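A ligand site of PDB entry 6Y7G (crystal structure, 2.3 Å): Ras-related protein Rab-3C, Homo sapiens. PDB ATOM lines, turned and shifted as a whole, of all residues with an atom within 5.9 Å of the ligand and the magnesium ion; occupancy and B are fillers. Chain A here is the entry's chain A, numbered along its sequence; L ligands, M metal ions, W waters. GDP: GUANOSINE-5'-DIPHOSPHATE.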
ATOM      1  N   GLY A  37     -25.652 -35.537  -4.852  1.00  0.00           N
ATOM      2  CA  GLY A  37     -26.209 -34.200  -4.602  1.00  0.00           C
ATOM      3  C   GLY A  37     -27.551 -34.029  -5.291  1.00  0.00           C
ATOM      4  O   GLY A  37     -27.816 -34.777  -6.241  1.00  0.00           O
ATOM      5  N   ASN A  38     -28.291 -33.010  -4.882  1.00  0.00           N
ATOM      6  CA  ASN A  38     -29.623 -32.692  -5.442  1.00  0.00           C
ATOM      7  C   ASN A  38     -29.553 -32.506  -6.960  1.00  0.00           C
ATOM      8  O   ASN A  38     -28.562 -32.021  -7.504  1.00  0.00           O
ATOM      9  CB  ASN A  38     -30.165 -31.408  -4.837  1.00  0.00           C
ATOM     10  CG  ASN A  38     -30.729 -31.566  -3.448  1.00  0.00           C
ATOM     11  OD1 ASN A  38     -30.286 -32.386  -2.676  1.00  0.00           O
ATOM     12  ND2 ASN A  38     -31.716 -30.745  -3.113  1.00  0.00           N
ATOM     13  N   SER A  39     -30.691 -32.635  -7.618  1.00  0.00           N
ATOM     14  CA  SER A  39     -30.759 -32.427  -9.079  1.00  0.00           C
ATOM     15  C   SER A  39     -30.522 -30.946  -9.405  1.00  0.00           C
ATOM     16  O   SER A  39     -30.895 -30.126  -8.523  1.00  0.00           O
ATOM     17  CB  SER A  39     -32.089 -32.872  -9.628  1.00  0.00           C
ATOM     18  OG  SER A  39     -33.068 -33.028  -8.616  1.00  0.00           O
ATOM     19  N   SER A  40     -29.864 -30.690 -10.574  1.00  0.00           N
ATOM     20  CA  SER A  40     -29.592 -29.367 -11.208  1.00  0.00           C
ATOM     21  C   SER A  40     -28.353 -28.674 -10.632  1.00  0.00           C
ATOM     22  O   SER A  40     -28.029 -27.569 -11.104  1.00  0.00           O
ATOM     23  CB  SER A  40     -30.806 -28.459 -11.143  1.00  0.00           C
ATOM     24  OG  SER A  40     -31.743 -28.815 -12.160  1.00  0.00           O
ATOM     25  N   VAL A  41     -27.635 -29.294  -9.690  1.00  0.00           N
ATOM     26  CA  VAL A  41     -26.419 -28.700  -9.050  1.00  0.00           C
ATOM     27  C   VAL A  41     -25.213 -28.799  -9.993  1.00  0.00           C
ATOM     28  O   VAL A  41     -24.263 -28.035  -9.782  1.00  0.00           O
ATOM     29  CB  VAL A  41     -26.135 -29.329  -7.670  1.00  0.00           C
ATOM     30  CG1 VAL A  41     -27.313 -29.153  -6.742  1.00  0.00           C
ATOM     31  CG2 VAL A  41     -25.698 -30.793  -7.734  1.00  0.00           C
ATOM     32  N   GLY A  42     -25.259 -29.675 -10.997  1.00  0.00           N
ATOM     33  CA  GLY A  42     -24.239 -29.728 -12.068  1.00  0.00           C
ATOM     34  C   GLY A  42     -23.425 -31.006 -12.056  1.00  0.00           C
ATOM     35  O   GLY A  42     -22.314 -30.998 -12.628  1.00  0.00           O
ATOM     36  N   LYS A  43     -23.962 -32.077 -11.477  1.00  0.00           N
ATOM     37  CA  LYS A  43     -23.302 -33.393 -11.345  1.00  0.00           C
ATOM     38  C   LYS A  43     -22.861 -33.905 -12.719  1.00  0.00           C
ATOM     39  O   LYS A  43     -21.669 -34.258 -12.895  1.00  0.00           O
ATOM     40  CB  LYS A  43     -24.275 -34.372 -10.694  1.00  0.00           C
ATOM     41  CG  LYS A  43     -24.643 -34.057  -9.249  1.00  0.00           C
ATOM     42  CD  LYS A  43     -25.467 -35.152  -8.614  1.00  0.00           C
ATOM     43  CE  LYS A  43     -26.833 -35.323  -9.252  1.00  0.00           C
ATOM     44  NZ  LYS A  43     -27.692 -34.135  -9.071  1.00  0.00           N
ATOM     45  N   THR A  44     -23.796 -33.929 -13.672  1.00  0.00           N
ATOM     46  CA  THR A  44     -23.590 -34.440 -15.062  1.00  0.00           C
ATOM     47  C   THR A  44     -22.579 -33.538 -15.778  1.00  0.00           C
ATOM     48  O   THR A  44     -21.667 -34.082 -16.434  1.00  0.00           O
ATOM     49  CB  THR A  44     -24.953 -34.591 -15.753  1.00  0.00           C
ATOM     50  OG1 THR A  44     -25.770 -35.428 -14.935  1.00  0.00           O
ATOM     51  CG2 THR A  44     -24.861 -35.184 -17.151  1.00  0.00           C
ATOM     52  N   SER A  45     -22.710 -32.219 -15.653  1.00  0.00           N
ATOM     53  CA  SER A  45     -21.804 -31.239 -16.309  1.00  0.00           C
ATOM     54  C   SER A  45     -20.393 -31.398 -15.753  1.00  0.00           C
ATOM     55  O   SER A  45     -19.416 -31.371 -16.530  1.00  0.00           O
ATOM     56  CB  SER A  45     -22.313 -29.847 -16.126  1.00  0.00           C
ATOM     57  OG  SER A  45     -23.712 -29.781 -16.373  1.00  0.00           O
ATOM     58  N   PHE A  46     -20.276 -31.570 -14.426  1.00  0.00           N
ATOM     59  CA  PHE A  46     -18.977 -31.754 -13.732  1.00  0.00           C
ATOM     60  C   PHE A  46     -18.288 -32.961 -14.354  1.00  0.00           C
ATOM     61  O   PHE A  46     -17.130 -32.844 -14.772  1.00  0.00           O
ATOM     62  CB  PHE A  46     -19.224 -31.898 -12.238  1.00  0.00           C
ATOM     63  CG  PHE A  46     -18.046 -31.610 -11.354  1.00  0.00           C
ATOM     64  CD1 PHE A  46     -17.779 -30.308 -10.944  1.00  0.00           C
ATOM     65  CD2 PHE A  46     -17.241 -32.636 -10.873  1.00  0.00           C
ATOM     66  CE1 PHE A  46     -16.723 -30.049 -10.080  1.00  0.00           C
ATOM     67  CE2 PHE A  46     -16.170 -32.359 -10.035  1.00  0.00           C
ATOM     68  CZ  PHE A  46     -15.903 -31.067  -9.647  1.00  0.00           C
ATOM     69  N   PHE A  55     -18.307 -28.542 -22.129  1.00  0.00           N
ATOM     70  CA  PHE A  55     -19.556 -28.072 -21.467  1.00  0.00           C
ATOM     71  C   PHE A  55     -20.415 -27.405 -22.533  1.00  0.00           C
ATOM     72  O   PHE A  55     -19.834 -26.757 -23.429  1.00  0.00           O
ATOM     73  CB  PHE A  55     -19.223 -27.128 -20.320  1.00  0.00           C
ATOM     74  CG  PHE A  55     -20.406 -26.414 -19.725  1.00  0.00           C
ATOM     75  CD1 PHE A  55     -20.853 -25.214 -20.254  1.00  0.00           C
ATOM     76  CD2 PHE A  55     -21.064 -26.933 -18.614  1.00  0.00           C
ATOM     77  CE1 PHE A  55     -21.941 -24.556 -19.701  1.00  0.00           C
ATOM     78  CE2 PHE A  55     -22.143 -26.275 -18.065  1.00  0.00           C
ATOM     79  CZ  PHE A  55     -22.583 -25.087 -18.598  1.00  0.00           C
ATOM     80  N   THR A  56     -21.735 -27.595 -22.458  1.00  0.00           N
ATOM     81  CA  THR A  56     -22.710 -27.043 -23.415  1.00  0.00           C
ATOM     82  C   THR A  56     -23.942 -26.569 -22.630  1.00  0.00           C
ATOM     83  O   THR A  56     -24.444 -27.340 -21.788  1.00  0.00           O
ATOM     84  CB  THR A  56     -23.071 -28.054 -24.525  1.00  0.00           C
ATOM     85  OG1 THR A  56     -24.137 -28.889 -24.051  1.00  0.00           O
ATOM     86  CG2 THR A  56     -21.910 -28.912 -24.953  1.00  0.00           C
ATOM     87  N   SER A  57     -24.386 -25.347 -22.920  1.00  0.00           N
ATOM     88  CA  SER A  57     -25.685 -24.770 -22.477  1.00  0.00           C
ATOM     89  C   SER A  57     -26.833 -25.569 -23.110  1.00  0.00           C
ATOM     90  O   SER A  57     -27.971 -25.469 -22.592  1.00  0.00           O
ATOM     91  CB  SER A  57     -25.758 -23.305 -22.834  1.00  0.00           C
ATOM     92  OG  SER A  57     -24.528 -22.653 -22.560  1.00  0.00           O
ATOM     93  N   ASP A  85     -22.554 -41.241 -12.259  1.00  0.00           N
ATOM     94  CA  ASP A  85     -23.473 -40.069 -12.218  1.00  0.00           C
ATOM     95  C   ASP A  85     -24.910 -40.582 -12.225  1.00  0.00           C
ATOM     96  O   ASP A  85     -25.633 -40.346 -13.214  1.00  0.00           O
ATOM     97  CB  ASP A  85     -23.169 -39.172 -13.413  1.00  0.00           C
ATOM     98  CG  ASP A  85     -24.071 -37.966 -13.559  1.00  0.00           C
ATOM     99  OD1 ASP A  85     -24.449 -37.393 -12.537  1.00  0.00           O
ATOM    100  OD2 ASP A  85     -24.405 -37.620 -14.709  1.00  0.00           O
ATOM    101  N   MET A 109     -21.914 -32.702  -4.125  1.00  0.00           N
ATOM    102  CA  MET A 109     -22.130 -31.425  -4.843  1.00  0.00           C
ATOM    103  C   MET A 109     -23.389 -30.706  -4.304  1.00  0.00           C
ATOM    104  O   MET A 109     -24.428 -31.354  -4.135  1.00  0.00           O
ATOM    105  CB  MET A 109     -22.307 -31.674  -6.339  1.00  0.00           C
ATOM    106  CG  MET A 109     -21.001 -32.000  -7.052  1.00  0.00           C
ATOM    107  SD  MET A 109     -21.041 -31.686  -8.837  1.00  0.00           S
ATOM    108  CE  MET A 109     -22.094 -30.243  -8.912  1.00  0.00           C
ATOM    109  N   ASN A 143     -20.660 -25.954  -6.479  1.00  0.00           N
ATOM    110  CA  ASN A 143     -20.611 -25.756  -7.944  1.00  0.00           C
ATOM    111  C   ASN A 143     -21.254 -24.425  -8.362  1.00  0.00           C
ATOM    112  O   ASN A 143     -22.010 -23.891  -7.584  1.00  0.00           O
ATOM    113  CB  ASN A 143     -21.253 -26.954  -8.651  1.00  0.00           C
ATOM    114  CG  ASN A 143     -20.833 -27.096 -10.089  1.00  0.00           C
ATOM    115  OD1 ASN A 143     -21.661 -27.292 -10.949  1.00  0.00           O
ATOM    116  ND2 ASN A 143     -19.579 -26.827 -10.357  1.00  0.00           N
ATOM    117  N   LYS A 144     -20.899 -23.943  -9.563  1.00  0.00           N
ATOM    118  CA  LYS A 144     -21.384 -22.731 -10.269  1.00  0.00           C
ATOM    119  C   LYS A 144     -20.811 -21.478  -9.648  1.00  0.00           C
ATOM    120  O   LYS A 144     -21.528 -20.535  -9.558  1.00  0.00           O
ATOM    121  CB  LYS A 144     -22.905 -22.658 -10.392  1.00  0.00           C
ATOM    122  CG  LYS A 144     -23.595 -23.948 -10.776  1.00  0.00           C
ATOM    123  CD  LYS A 144     -25.012 -23.783 -11.189  1.00  0.00           C
ATOM    124  CE  LYS A 144     -25.706 -25.109 -11.381  1.00  0.00           C
ATOM    125  NZ  LYS A 144     -27.126 -24.915 -11.704  1.00  0.00           N
ATOM    126  N   CYS A 145     -19.539 -21.496  -9.273  1.00  0.00           N
ATOM    127  CA  CYS A 145     -18.909 -20.303  -8.648  1.00  0.00           C
ATOM    128  C   CYS A 145     -18.775 -19.179  -9.679  1.00  0.00           C
ATOM    129  O   CYS A 145     -18.387 -18.100  -9.284  1.00  0.00           O
ATOM    130  CB  CYS A 145     -17.582 -20.654  -7.981  1.00  0.00           C
ATOM    131  SG  CYS A 145     -16.362 -21.379  -9.098  1.00  0.00           S
ATOM    132  N   ASP A 146     -19.071 -19.476 -10.940  1.00  0.00           N
ATOM    133  CA  ASP A 146     -19.105 -18.483 -12.037  1.00  0.00           C
ATOM    134  C   ASP A 146     -20.319 -17.556 -11.927  1.00  0.00           C
ATOM    135  O   ASP A 146     -20.264 -16.461 -12.521  1.00  0.00           O
ATOM    136  CB  ASP A 146     -19.148 -19.155 -13.411  1.00  0.00           C
ATOM    137  CG  ASP A 146     -20.343 -20.071 -13.573  1.00  0.00           C
ATOM    138  OD1 ASP A 146     -20.351 -21.145 -12.899  1.00  0.00           O
ATOM    139  OD2 ASP A 146     -21.258 -19.707 -14.335  1.00  0.00           O
ATOM    140  N   MET A 147     -21.380 -17.993 -11.222  1.00  0.00           N
ATOM    141  CA  MET A 147     -22.666 -17.257 -11.081  1.00  0.00           C
ATOM    142  C   MET A 147     -22.622 -16.410  -9.798  1.00  0.00           C
ATOM    143  O   MET A 147     -23.452 -16.638  -8.904  1.00  0.00           O
ATOM    144  CB  MET A 147     -23.841 -18.223 -11.040  1.00  0.00           C
ATOM    145  CG  MET A 147     -23.900 -19.141 -12.249  1.00  0.00           C
ATOM    146  SD  MET A 147     -24.268 -18.240 -13.785  1.00  0.00           S
ATOM    147  CE  MET A 147     -25.991 -17.838 -13.538  1.00  0.00           C
ATOM    148  N   THR A 172     -16.319 -24.666  -7.419  1.00  0.00           N
ATOM    149  CA  THR A 172     -16.077 -25.143  -8.788  1.00  0.00           C
ATOM    150  C   THR A 172     -17.073 -24.506  -9.750  1.00  0.00           C
ATOM    151  O   THR A 172     -18.095 -24.008  -9.293  1.00  0.00           O
ATOM    152  CB  THR A 172     -16.211 -26.670  -8.917  1.00  0.00           C
ATOM    153  OG1 THR A 172     -17.593 -27.013  -8.800  1.00  0.00           O
ATOM    154  CG2 THR A 172     -15.388 -27.441  -7.900  1.00  0.00           C
ATOM    155  N   SER A 173     -16.765 -24.643 -11.036  1.00  0.00           N
ATOM    156  CA  SER A 173     -17.630 -24.337 -12.189  1.00  0.00           C
ATOM    157  C   SER A 173     -17.325 -25.341 -13.299  1.00  0.00           C
ATOM    158  O   SER A 173     -16.176 -25.351 -13.824  1.00  0.00           O
ATOM    159  CB  SER A 173     -17.410 -22.919 -12.665  1.00  0.00           C
ATOM    160  OG  SER A 173     -18.161 -22.653 -13.844  1.00  0.00           O
ATOM    161  N   ALA A 174     -18.293 -26.190 -13.630  1.00  0.00           N
ATOM    162  CA  ALA A 174     -18.249 -27.076 -14.811  1.00  0.00           C
ATOM    163  C   ALA A 174     -18.175 -26.188 -16.057  1.00  0.00           C
ATOM    164  O   ALA A 174     -17.525 -26.596 -17.039  1.00  0.00           O
ATOM    165  CB  ALA A 174     -19.451 -27.985 -14.808  1.00  0.00           C
ATOM    166  N   LYS A 175     -18.767 -24.982 -15.979  1.00  0.00           N
ATOM    167  CA  LYS A 175     -18.991 -24.037 -17.093  1.00  0.00           C
ATOM    168  C   LYS A 175     -17.697 -23.335 -17.464  1.00  0.00           C
ATOM    169  O   LYS A 175     -17.294 -23.420 -18.642  1.00  0.00           O
ATOM    170  CB  LYS A 175     -20.052 -23.003 -16.676  1.00  0.00           C
ATOM    171  CG  LYS A 175     -20.468 -22.025 -17.766  1.00  0.00           C
ATOM    172  CD  LYS A 175     -21.751 -21.306 -17.423  1.00  0.00           C
ATOM    173  CE  LYS A 175     -22.267 -20.462 -18.573  1.00  0.00           C
ATOM    174  NZ  LYS A 175     -21.193 -19.567 -19.077  1.00  0.00           N
ATOM    175  N   ASP A 176     -17.061 -22.692 -16.496  1.00  0.00           N
ATOM    176  CA  ASP A 176     -15.778 -21.964 -16.688  1.00  0.00           C
ATOM    177  C   ASP A 176     -14.568 -22.870 -16.439  1.00  0.00           C
ATOM    178  O   ASP A 176     -13.437 -22.342 -16.548  1.00  0.00           O
ATOM    179  CB  ASP A 176     -15.696 -20.726 -15.792  1.00  0.00           C
ATOM    180  CG  ASP A 176     -16.646 -19.615 -16.208  1.00  0.00           C
ATOM    181  OD1 ASP A 176     -17.305 -19.774 -17.260  1.00  0.00           O
ATOM    182  OD2 ASP A 176     -16.727 -18.598 -15.463  1.00  0.00           O
HETATM  183  PB  GDP L   1     -27.436 -32.411 -12.516  1.00  0.00           P
HETATM  184  O1B GDP L   1     -26.767 -33.464 -13.407  1.00  0.00           O
HETATM  185  O2B GDP L   1     -28.925 -32.550 -12.500  1.00  0.00           O
HETATM  186  O3B GDP L   1     -26.951 -32.294 -11.067  1.00  0.00           O
HETATM  187  O3A GDP L   1     -27.135 -30.961 -13.182  1.00  0.00           O
HETATM  188  PA  GDP L   1     -26.699 -30.746 -14.721  1.00  0.00           P
HETATM  189  O1A GDP L   1     -27.684 -31.516 -15.555  1.00  0.00           O
HETATM  190  O2A GDP L   1     -25.223 -31.107 -14.922  1.00  0.00           O
HETATM  191  O5' GDP L   1     -26.820 -29.166 -14.919  1.00  0.00           O
HETATM  192  C5' GDP L   1     -27.922 -28.454 -14.367  1.00  0.00           C
HETATM  193  C4' GDP L   1     -28.028 -27.048 -14.944  1.00  0.00           C
HETATM  194  O4' GDP L   1     -27.032 -26.171 -14.395  1.00  0.00           O
HETATM  195  C3' GDP L   1     -27.819 -27.049 -16.447  1.00  0.00           C
HETATM  196  O3' GDP L   1     -28.575 -25.968 -17.018  1.00  0.00           O
HETATM  197  C2' GDP L   1     -26.345 -26.771 -16.607  1.00  0.00           C
HETATM  198  O2' GDP L   1     -25.982 -26.197 -17.878  1.00  0.00           O
HETATM  199  C1' GDP L   1     -26.102 -25.813 -15.444  1.00  0.00           C
HETATM  200  N9  GDP L   1     -24.736 -25.902 -14.918  1.00  0.00           N
HETATM  201  C8  GDP L   1     -24.040 -27.027 -14.587  1.00  0.00           C
HETATM  202  N7  GDP L   1     -22.807 -26.696 -14.098  1.00  0.00           N
HETATM  203  C5  GDP L   1     -22.722 -25.350 -14.097  1.00  0.00           C
HETATM  204  C6  GDP L   1     -21.707 -24.339 -13.715  1.00  0.00           C
HETATM  205  O6  GDP L   1     -20.590 -24.657 -13.255  1.00  0.00           O
HETATM  206  N1  GDP L   1     -22.031 -23.049 -13.895  1.00  0.00           N
HETATM  207  C2  GDP L   1     -23.234 -22.674 -14.403  1.00  0.00           C
HETATM  208  N2  GDP L   1     -23.509 -21.353 -14.555  1.00  0.00           N
HETATM  209  N3  GDP L   1     -24.213 -23.519 -14.761  1.00  0.00           N
HETATM  210  C4  GDP L   1     -24.004 -24.838 -14.637  1.00  0.00           C
HETATM  211 MG    MG M   1     -27.797 -35.416 -14.155  1.00  0.00          MG
HETATM  212  O   HOH W   1     -29.541 -34.940 -13.235  1.00  0.00           O
HETATM  213  O   HOH W   2     -24.597 -28.328 -19.109  1.00  0.00           O
HETATM  214  O   HOH W   3     -27.988 -33.967 -15.685  1.00  0.00           O
HETATM  215  O   HOH W   4     -26.853 -36.619 -12.667  1.00  0.00           O
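The side-chain amide oxygen of Asn 143 lies close to a nitrogen (N7) of the ligand (3.4 Å).
O2A of the ligand is in hydrogen-bond range of OG of Ser 45, 2.5 Å away.
The backbone NH of Ser 40 lies within hydrogen-bond range of an oxygen (O2B) of the ligand.
O3B of the ligand is in salt-bridge range of NZ of Lys 43 (2.8 Å).
The backbone NH of Ala 174 sits at hydrogen-bond distance from an oxygen (O6) of the ligand (2.8 Å).
The backbone NH (N) of Gly 42 sits at hydrogen-bond distance from an oxygen (O3B) of the ligand, at 3.1 Å.
A nitrogen (N2) of the ligand sits close to the side-chain sulfur (SD) of Met 147.
OG of Ser 173 lies close to O6 of the ligand (3.2 Å).
A nitrogen (N1) of the ligand is in hydrogen-bond range of the side-chain carboxylate of Asp 146.
An oxygen (O3B) of the ligand lies within hydrogen-bond range of the backbone NH (N) of Val 41, at 3.4 Å.
An oxygen (O3B) of the ligand lies within hydrogen-bond range of the backbone NH (N) of Lys 43 (3.0 Å).
The backbone NH of Thr 44 sits at hydrogen-bond distance from an oxygen (O2A) of the ligand (3.4 Å).
The side-chain amino group of Lys 144 sits at hydrogen-bond distance from an oxygen (O4') of the ligand.
The backbone NH (N) of Ser 45 sits at hydrogen-bond distance from an oxygen (O2A) of the ligand.
N of Lys 175 is in hydrogen-bond range of O6 of the ligand (3.3 Å).
Water W2 lies within hydrogen-bond range of an oxygen (O2') of the ligand (2.8 Å), the backbone carbonyl oxygen (O) of Thr 56 (2.9 Å) and the side-chain hydroxyl (OG) of Ser 45 (3.2 Å).
Merely in contact with the ligand: Asn 38, Ser 39 and Phe 55.
Hydrophobic or aromatic side chains that line the ligand: Val 41, Phe 55, Met 147 and Ala 174.
16 residues have an atom within 4 Å of the ligand: Asn 38, Ser 39, Ser 40, Val 41, Gly 42, Lys 43, Thr 44, Ser 45, Phe 55, Asn 143, Lys 144, Asp 146, Met 147, Ser 173, Ala 174 and Lys 175.
The side-chain amide nitrogen (ND2) of Asn 143 sits at hydrogen-bond distance from the side-chain hydroxyl (OG1) of Thr 172, at 2.5 Å.
The side-chain amino group (NZ) of Lys 43 sits at hydrogen-bond distance from the backbone carbonyl oxygen (O) of Asn 38, 2.8 Å away.
The side-chain hydroxyl (OG) of Ser 173 lies close to the backbone NH (N) of Lys 175, 3.2 Å away.
The side-chain hydroxyl (OG) of Ser 173 is in hydrogen-bond range of the side-chain carboxylate (OD1) of Asp 146, 2.8 Å away.
The side-chain amino group (NZ) of Lys 43 is in hydrogen-bond range of the backbone carbonyl oxygen (O) of Gly 37 (2.9 Å).
The side-chain amino group (NZ) of Lys 144 is in hydrogen-bond range of the backbone carbonyl oxygen (O) of Ser 40, at 2.9 Å.
O of Thr 172 lies within hydrogen-bond range of N of Lys 144, at 2.8 Å.
O of Val 41 lies close to OD1 of Asn 143, 2.9 Å away.
The magnesium ion is bound by water W1 (2.0 Å), water W3 (2.1 Å), water W4 (2.1 Å), the side-chain hydroxyl of Thr 44 (2.2 Å) and an oxygen (O1B) of the ligand (2.3 Å).
The magnesium ion has five donor atoms within binding distance.
Of the 25 residues printed, 1 comes within 4 Å of the magnesium ion.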
